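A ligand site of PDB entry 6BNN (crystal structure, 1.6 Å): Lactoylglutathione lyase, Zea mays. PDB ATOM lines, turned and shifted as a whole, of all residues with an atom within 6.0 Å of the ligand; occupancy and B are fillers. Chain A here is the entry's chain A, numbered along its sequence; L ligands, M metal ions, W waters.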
ATOM      1  N   GLY A 101      17.812  -3.626   2.287  1.00  0.00           N
ATOM      2  CA  GLY A 101      18.768  -2.524   2.002  1.00  0.00           C
ATOM      3  C   GLY A 101      18.252  -1.178   2.545  1.00  0.00           C
ATOM      4  O   GLY A 101      18.714  -0.657   3.567  1.00  0.00           O
ATOM      5  N   HIS A 102      17.360  -0.561   1.772  1.00  0.00           N
ATOM      6  CA  HIS A 102      16.886   0.780   2.129  1.00  0.00           C
ATOM      7  C   HIS A 102      15.705   1.115   1.260  1.00  0.00           C
ATOM      8  O   HIS A 102      15.417   0.440   0.263  1.00  0.00           O
ATOM      9  CB  HIS A 102      17.949   1.858   1.914  1.00  0.00           C
ATOM     10  CG  HIS A 102      18.606   1.869   0.559  1.00  0.00           C
ATOM     11  ND1 HIS A 102      19.884   1.375   0.349  1.00  0.00           N
ATOM     12  CD2 HIS A 102      18.209   2.394  -0.620  1.00  0.00           C
ATOM     13  CE1 HIS A 102      20.217   1.570  -0.914  1.00  0.00           C
ATOM     14  NE2 HIS A 102      19.231   2.218  -1.522  1.00  0.00           N
ATOM     15  N   ARG A 126      25.060   8.999   7.038  1.00  0.00           N
ATOM     16  CA  ARG A 126      25.991   9.223   5.965  1.00  0.00           C
ATOM     17  C   ARG A 126      25.706  10.624   5.498  1.00  0.00           C
ATOM     18  O   ARG A 126      24.648  10.943   4.949  1.00  0.00           O
ATOM     19  CB  ARG A 126      25.825   8.144   4.852  1.00  0.00           C
ATOM     20  CG  ARG A 126      26.986   7.939   3.893  1.00  0.00           C
ATOM     21  CD  ARG A 126      27.009   8.973   2.783  1.00  0.00           C
ATOM     22  NE  ARG A 126      27.848   8.619   1.624  1.00  0.00           N
ATOM     23  CZ  ARG A 126      28.016   9.414   0.578  1.00  0.00           C
ATOM     24  NH1 ARG A 126      27.400  10.608   0.517  1.00  0.00           N
ATOM     25  NH2 ARG A 126      28.816   9.033  -0.404  1.00  0.00           N
ATOM     26  N   PRO A 130      28.845  13.292  -3.015  1.00  0.00           N
ATOM     27  CA  PRO A 130      28.823  12.327  -4.144  1.00  0.00           C
ATOM     28  C   PRO A 130      29.011  10.880  -3.707  1.00  0.00           C
ATOM     29  O   PRO A 130      29.684  10.635  -2.707  1.00  0.00           O
ATOM     30  CB  PRO A 130      30.000  12.794  -5.045  1.00  0.00           C
ATOM     31  CG  PRO A 130      30.141  14.251  -4.687  1.00  0.00           C
ATOM     32  CD  PRO A 130      29.902  14.303  -3.203  1.00  0.00           C
ATOM     33  N   VAL A 131      28.381   9.949  -4.407  1.00  0.00           N
ATOM     34  CA  VAL A 131      28.534   8.521  -4.085  1.00  0.00           C
ATOM     35  C   VAL A 131      29.994   8.146  -4.382  1.00  0.00           C
ATOM     36  O   VAL A 131      30.608   8.699  -5.309  1.00  0.00           O
ATOM     37  CB  VAL A 131      27.453   7.613  -4.757  1.00  0.00           C
ATOM     38  CG1 VAL A 131      27.551   7.618  -6.282  1.00  0.00           C
ATOM     39  CG2 VAL A 131      27.529   6.181  -4.221  1.00  0.00           C
ATOM     40  N   LYS A 132      30.567   7.287  -3.540  1.00  0.00           N
ATOM     41  CA  LYS A 132      31.989   6.946  -3.621  1.00  0.00           C
ATOM     42  C   LYS A 132      32.341   6.392  -5.013  1.00  0.00           C
ATOM     43  O   LYS A 132      31.844   5.329  -5.411  1.00  0.00           O
ATOM     44  CB  LYS A 132      32.366   5.929  -2.523  1.00  0.00           C
ATOM     45  CG  LYS A 132      32.413   6.470  -1.109  1.00  0.00           C
ATOM     46  CD  LYS A 132      32.986   5.395  -0.186  1.00  0.00           C
ATOM     47  CE  LYS A 132      32.519   5.563   1.251  1.00  0.00           C
ATOM     48  NZ  LYS A 132      33.118   6.748   1.926  1.00  0.00           N
ATOM     49  N   ILE A 138      24.296  11.921  -2.605  1.00  0.00           N
ATOM     50  CA  ILE A 138      23.420  11.066  -1.801  1.00  0.00           C
ATOM     51  C   ILE A 138      23.691  11.346  -0.329  1.00  0.00           C
ATOM     52  O   ILE A 138      24.774  11.902   0.011  1.00  0.00           O
ATOM     53  CB  ILE A 138      23.596   9.535  -2.080  1.00  0.00           C
ATOM     54  CG1 ILE A 138      25.019   9.020  -1.719  1.00  0.00           C
ATOM     55  CG2 ILE A 138      23.224   9.148  -3.527  1.00  0.00           C
ATOM     56  CD1 ILE A 138      24.933   7.577  -1.327  1.00  0.00           C
ATOM     57  N   PHE A 140      22.450   9.252   3.777  1.00  0.00           N
ATOM     58  CA  PHE A 140      21.569   8.253   4.381  1.00  0.00           C
ATOM     59  C   PHE A 140      21.039   8.694   5.744  1.00  0.00           C
ATOM     60  O   PHE A 140      21.733   9.339   6.548  1.00  0.00           O
ATOM     61  CB  PHE A 140      22.285   6.911   4.606  1.00  0.00           C
ATOM     62  CG  PHE A 140      22.335   6.016   3.391  1.00  0.00           C
ATOM     63  CD1 PHE A 140      23.396   6.100   2.483  1.00  0.00           C
ATOM     64  CD2 PHE A 140      21.331   5.064   3.179  1.00  0.00           C
ATOM     65  CE1 PHE A 140      23.444   5.243   1.349  1.00  0.00           C
ATOM     66  CE2 PHE A 140      21.381   4.210   2.058  1.00  0.00           C
ATOM     67  CZ  PHE A 140      22.429   4.295   1.145  1.00  0.00           C
ATOM     68  N   GLU A 150      17.955   6.087   1.901  1.00  0.00           N
ATOM     69  CA  GLU A 150      18.843   6.833   1.056  1.00  0.00           C
ATOM     70  C   GLU A 150      18.146   8.106   0.602  1.00  0.00           C
ATOM     71  O   GLU A 150      16.981   8.071   0.206  1.00  0.00           O
ATOM     72  CB  GLU A 150      19.203   5.995  -0.174  1.00  0.00           C
ATOM     73  CG  GLU A 150      20.376   6.547  -1.002  1.00  0.00           C
ATOM     74  CD  GLU A 150      20.722   5.666  -2.187  1.00  0.00           C
ATOM     75  OE1 GLU A 150      19.873   4.856  -2.617  1.00  0.00           O
ATOM     76  OE2 GLU A 150      21.798   5.888  -2.758  1.00  0.00           O
ATOM     77  N   MET A 165      15.441  -1.112  -2.017  1.00  0.00           N
ATOM     78  CA  MET A 165      16.728  -1.819  -2.308  1.00  0.00           C
ATOM     79  C   MET A 165      16.797  -3.053  -1.450  1.00  0.00           C
ATOM     80  O   MET A 165      16.640  -2.973  -0.206  1.00  0.00           O
ATOM     81  CB  MET A 165      17.947  -0.909  -2.045  1.00  0.00           C
ATOM     82  CG  MET A 165      19.254  -1.595  -2.559  1.00  0.00           C
ATOM     83  SD  MET A 165      19.983  -2.906  -1.523  1.00  0.00           S
ATOM     84  CE  MET A 165      21.183  -1.986  -0.486  1.00  0.00           C
ATOM     85  N   ARG A 167      19.027  -6.893  -0.962  1.00  0.00           N
ATOM     86  CA  ARG A 167      20.223  -7.602  -1.363  1.00  0.00           C
ATOM     87  C   ARG A 167      19.872  -9.039  -1.855  1.00  0.00           C
ATOM     88  O   ARG A 167      18.932  -9.707  -1.327  1.00  0.00           O
ATOM     89  CB  ARG A 167      21.217  -7.663  -0.140  1.00  0.00           C
ATOM     90  CG  ARG A 167      21.596  -6.285   0.337  1.00  0.00           C
ATOM     91  CD  ARG A 167      22.569  -6.423   1.547  1.00  0.00           C
ATOM     92  NE  ARG A 167      22.883  -5.045   1.887  1.00  0.00           N
ATOM     93  CZ  ARG A 167      22.197  -4.300   2.771  1.00  0.00           C
ATOM     94  NH1 ARG A 167      21.290  -4.839   3.540  1.00  0.00           N
ATOM     95  NH2 ARG A 167      22.484  -2.991   2.881  1.00  0.00           N
ATOM     96  N   LYS A 190      25.331  -1.926 -12.765  1.00  0.00           N
ATOM     97  CA  LYS A 190      26.590  -1.213 -12.511  1.00  0.00           C
ATOM     98  C   LYS A 190      27.445  -2.052 -11.586  1.00  0.00           C
ATOM     99  O   LYS A 190      27.031  -2.338 -10.485  1.00  0.00           O
ATOM    100  CB  LYS A 190      26.343   0.168 -11.908  1.00  0.00           C
ATOM    101  CG  LYS A 190      27.648   0.922 -11.718  1.00  0.00           C
ATOM    102  CD  LYS A 190      27.456   2.413 -11.445  1.00  0.00           C
ATOM    103  CE  LYS A 190      26.963   2.684 -10.043  1.00  0.00           C
ATOM    104  NZ  LYS A 190      26.035   3.864 -10.047  1.00  0.00           N
ATOM    105  N   TYR A 195      34.671  -1.585  -4.548  1.00  0.00           N
ATOM    106  CA  TYR A 195      33.963  -1.786  -3.292  1.00  0.00           C
ATOM    107  C   TYR A 195      33.191  -3.147  -3.285  1.00  0.00           C
ATOM    108  O   TYR A 195      32.385  -3.404  -2.396  1.00  0.00           O
ATOM    109  CB  TYR A 195      33.020  -0.596  -3.027  1.00  0.00           C
ATOM    110  CG  TYR A 195      33.776   0.695  -2.847  1.00  0.00           C
ATOM    111  CD1 TYR A 195      34.482   0.944  -1.652  1.00  0.00           C
ATOM    112  CD2 TYR A 195      33.830   1.642  -3.860  1.00  0.00           C
ATOM    113  CE1 TYR A 195      35.189   2.128  -1.476  1.00  0.00           C
ATOM    114  CE2 TYR A 195      34.552   2.833  -3.702  1.00  0.00           C
ATOM    115  CZ  TYR A 195      35.223   3.064  -2.499  1.00  0.00           C
ATOM    116  OH  TYR A 195      35.943   4.233  -2.301  1.00  0.00           O
ATOM    117  N   TYR A 197      30.862  -4.744  -4.998  1.00  0.00           N
ATOM    118  CA  TYR A 197      29.419  -4.928  -5.180  1.00  0.00           C
ATOM    119  C   TYR A 197      29.008  -4.646  -6.619  1.00  0.00           C
ATOM    120  O   TYR A 197      29.766  -3.993  -7.387  1.00  0.00           O
ATOM    121  CB  TYR A 197      28.619  -4.127  -4.167  1.00  0.00           C
ATOM    122  CG  TYR A 197      28.579  -2.629  -4.385  1.00  0.00           C
ATOM    123  CD1 TYR A 197      27.638  -2.051  -5.211  1.00  0.00           C
ATOM    124  CD2 TYR A 197      29.468  -1.799  -3.725  1.00  0.00           C
ATOM    125  CE1 TYR A 197      27.598  -0.680  -5.408  1.00  0.00           C
ATOM    126  CE2 TYR A 197      29.440  -0.418  -3.897  1.00  0.00           C
ATOM    127  CZ  TYR A 197      28.487   0.136  -4.731  1.00  0.00           C
ATOM    128  OH  TYR A 197      28.452   1.515  -4.887  1.00  0.00           O
ATOM    129  N   ILE A 199      25.186  -3.530  -8.729  1.00  0.00           N
ATOM    130  CA  ILE A 199      23.737  -3.248  -8.540  1.00  0.00           C
ATOM    131  C   ILE A 199      22.992  -3.376  -9.844  1.00  0.00           C
ATOM    132  O   ILE A 199      23.574  -3.247 -10.905  1.00  0.00           O
ATOM    133  CB  ILE A 199      23.485  -1.842  -7.905  1.00  0.00           C
ATOM    134  CG1 ILE A 199      24.003  -0.668  -8.772  1.00  0.00           C
ATOM    135  CG2 ILE A 199      24.071  -1.813  -6.512  1.00  0.00           C
ATOM    136  CD1 ILE A 199      22.959  -0.101  -9.734  1.00  0.00           C
ATOM    137  N   GLU A 214      15.951  -1.830  -6.571  1.00  0.00           N
ATOM    138  CA  GLU A 214      17.416  -1.824  -6.695  1.00  0.00           C
ATOM    139  C   GLU A 214      17.850  -3.108  -6.008  1.00  0.00           C
ATOM    140  O   GLU A 214      17.472  -3.355  -4.860  1.00  0.00           O
ATOM    141  CB  GLU A 214      18.051  -0.610  -5.993  1.00  0.00           C
ATOM    142  CG  GLU A 214      19.589  -0.566  -6.119  1.00  0.00           C
ATOM    143  CD  GLU A 214      20.203   0.613  -5.336  1.00  0.00           C
ATOM    144  OE1 GLU A 214      19.484   1.294  -4.596  1.00  0.00           O
ATOM    145  OE2 GLU A 214      21.428   0.803  -5.401  1.00  0.00           O
ATOM    146  N   THR A 216      21.086  -5.492  -4.915  1.00  0.00           N
ATOM    147  CA  THR A 216      22.551  -5.393  -4.671  1.00  0.00           C
ATOM    148  C   THR A 216      23.128  -6.803  -4.401  1.00  0.00           C
ATOM    149  O   THR A 216      22.620  -7.583  -3.566  1.00  0.00           O
ATOM    150  CB  THR A 216      22.785  -4.519  -3.403  1.00  0.00           C
ATOM    151  OG1 THR A 216      22.253  -3.186  -3.644  1.00  0.00           O
ATOM    152  CG2 THR A 216      24.242  -4.365  -3.117  1.00  0.00           C
ATOM    153  N   TYR A 217      24.188  -7.086  -5.117  1.00  0.00           N
ATOM    154  CA  TYR A 217      25.002  -8.289  -4.906  1.00  0.00           C
ATOM    155  C   TYR A 217      26.348  -7.835  -4.331  1.00  0.00           C
ATOM    156  O   TYR A 217      26.986  -6.910  -4.861  1.00  0.00           O
ATOM    157  CB  TYR A 217      25.183  -8.985  -6.260  1.00  0.00           C
ATOM    158  CG  TYR A 217      26.258 -10.074  -6.212  1.00  0.00           C
ATOM    159  CD1 TYR A 217      26.004 -11.286  -5.583  1.00  0.00           C
ATOM    160  CD2 TYR A 217      27.514  -9.832  -6.803  1.00  0.00           C
ATOM    161  CE1 TYR A 217      27.006 -12.292  -5.517  1.00  0.00           C
ATOM    162  CE2 TYR A 217      28.514 -10.864  -6.755  1.00  0.00           C
ATOM    163  CZ  TYR A 217      28.243 -12.024  -6.082  1.00  0.00           C
ATOM    164  OH  TYR A 217      29.253 -12.977  -6.012  1.00  0.00           O
ATOM    165  N   ASN A 218      26.731  -8.459  -3.184  1.00  0.00           N
ATOM    166  CA  ASN A 218      28.072  -8.265  -2.607  1.00  0.00           C
ATOM    167  C   ASN A 218      28.922  -9.489  -2.962  1.00  0.00           C
ATOM    168  O   ASN A 218      28.459 -10.615  -2.877  1.00  0.00           O
ATOM    169  CB  ASN A 218      27.889  -8.172  -1.087  1.00  0.00           C
ATOM    170  CG  ASN A 218      27.295  -6.824  -0.686  1.00  0.00           C
ATOM    171  OD1 ASN A 218      27.998  -5.827  -0.752  1.00  0.00           O
ATOM    172  ND2 ASN A 218      26.016  -6.788  -0.239  1.00  0.00           N
ATOM    173  N   TYR A 224      21.224 -14.043   2.737  1.00  0.00           N
ATOM    174  CA  TYR A 224      20.973 -12.992   3.758  1.00  0.00           C
ATOM    175  C   TYR A 224      19.774 -13.407   4.573  1.00  0.00           C
ATOM    176  O   TYR A 224      18.885 -14.150   4.065  1.00  0.00           O
ATOM    177  CB  TYR A 224      20.593 -11.654   3.076  1.00  0.00           C
ATOM    178  CG  TYR A 224      21.682 -11.098   2.244  1.00  0.00           C
ATOM    179  CD1 TYR A 224      21.811 -11.456   0.856  1.00  0.00           C
ATOM    180  CD2 TYR A 224      22.637 -10.220   2.793  1.00  0.00           C
ATOM    181  CE1 TYR A 224      22.858 -10.949   0.081  1.00  0.00           C
ATOM    182  CE2 TYR A 224      23.697  -9.723   2.004  1.00  0.00           C
ATOM    183  CZ  TYR A 224      23.809 -10.068   0.673  1.00  0.00           C
ATOM    184  OH  TYR A 224      24.838  -9.521  -0.091  1.00  0.00           O
HETATM  185  N1  LIG L   1      27.819  -3.555   0.863  1.00  0.00           N
HETATM  186  C1  LIG L   1      26.862  -2.537   0.355  1.00  0.00           C
HETATM  187  C2  LIG L   1      25.410  -2.930   0.637  1.00  0.00           C
HETATM  188  O1  LIG L   1      24.520  -2.124   1.039  1.00  0.00           O
HETATM  189  O2  LIG L   1      25.170  -4.154   0.571  1.00  0.00           O
HETATM  190  C3  LIG L   1      27.145  -2.407  -1.136  1.00  0.00           C
HETATM  191  C4  LIG L   1      26.236  -1.381  -1.825  1.00  0.00           C
HETATM  192  C5  LIG L   1      26.694   0.046  -1.599  1.00  0.00           C
HETATM  193  O3  LIG L   1      27.657   0.314  -0.854  1.00  0.00           O
HETATM  194  N2  LIG L   1      25.960   0.956  -2.277  1.00  0.00           N
HETATM  195  C6  LIG L   1      26.254   2.392  -2.312  1.00  0.00           C
HETATM  196  C7  LIG L   1      26.461   2.927  -0.912  1.00  0.00           C
HETATM  197  O4  LIG L   1      25.721   2.631   0.033  1.00  0.00           O
HETATM  198  C8  LIG L   1      25.241   3.250  -3.082  1.00  0.00           C
HETATM  199  S1  LIG L   1      24.801   2.536  -4.711  1.00  0.00           S
HETATM  200  N3  LIG L   1      27.540   3.683  -0.807  1.00  0.00           N
HETATM  201  C9  LIG L   1      27.912   4.337   0.422  1.00  0.00           C
HETATM  202  C10 LIG L   1      28.666   5.624   0.162  1.00  0.00           C
HETATM  203  O5  LIG L   1      28.683   6.128  -0.996  1.00  0.00           O
HETATM  204  O6  LIG L   1      29.245   6.146   1.147  1.00  0.00           O
HETATM  205 CO    CO M   1      19.766   2.991  -3.452  1.00  0.00          CO
HETATM  206  O   HOH W   1      23.294  -0.559  -3.149  1.00  0.00           O
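CG2 of Val 131 touches O5 of the ligand, 3.4 Å away. CE1 of Phe 140 touches O4 of the ligand (3.7 Å). Met 165 touches the ligand. Glu 214 touches the ligand. Thr 216 touches the ligand. Hydrophobic or aromatic side chains within 4 Å of the ligand: Val 131, Phe 140, Met 165 and Tyr 197. Ten residues have an atom within 4 Å of the ligand: Arg 126, Val 131, Lys 132, Phe 140, Met 165, Arg 167, Tyr 197, Glu 214, Thr 216 and Asn 218. The nearest printed residue that does not touch the ligand is Ile 138 (4.03 Å).
Water W1 lies within hydrogen-bond range of OG1 of Thr 216 (2.9 Å), N2 of the ligand (3.2 Å) and OE2 of Glu 214 (3.2 Å).
The side-chain amide nitrogen (ND2) of Asn 218 sits at hydrogen-bond distance from the side-chain hydroxyl (OH) of Tyr 224 (3.0 Å). The backbone carbonyl oxygen of Arg 126 sits at hydrogen-bond distance from the backbone NH of Phe 140 (3.0 Å). The guanidinium group (NH1) of Arg 126 sits at hydrogen-bond distance from the backbone carbonyl oxygen (O) of Ile 138, 3.0 Å away. O of Pro 130 sits at hydrogen-bond distance from NH2 of Arg 126, 2.9 Å away. SD of Met 165 sits at hydrogen-bond distance from OG1 of Thr 216 (3.1 Å). The backbone NH (N) of Met 165 is in hydrogen-bond range of the backbone carbonyl oxygen (O) of His 102, 2.8 Å away. The backbone carbonyl oxygen (O) of Met 165 sits at hydrogen-bond distance from the backbone NH (N) of Gly 101 (2.8 Å).
An oxygen (O2) of the ligand lies within salt-bridge range of the guanidinium group (NE) of Arg 167 (2.8 Å). The side-chain amide oxygen (OD1) of Asn 218 lies within hydrogen-bond range of a nitrogen (N1) of the ligand, at 2.8 Å. O6 of the ligand is in salt-bridge range of NE of Arg 126 (2.9 Å). An oxygen (O5) of the ligand is in hydrogen-bond range of the backbone NH (N) of Lys 132 (3.4 Å). The side-chain amino group of Lys 132 is in salt-bridge range of an oxygen (O6) of the ligand (3.996 Å). OH of Tyr 197 lies close to S1 of the ligand, at 3.8 Å.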
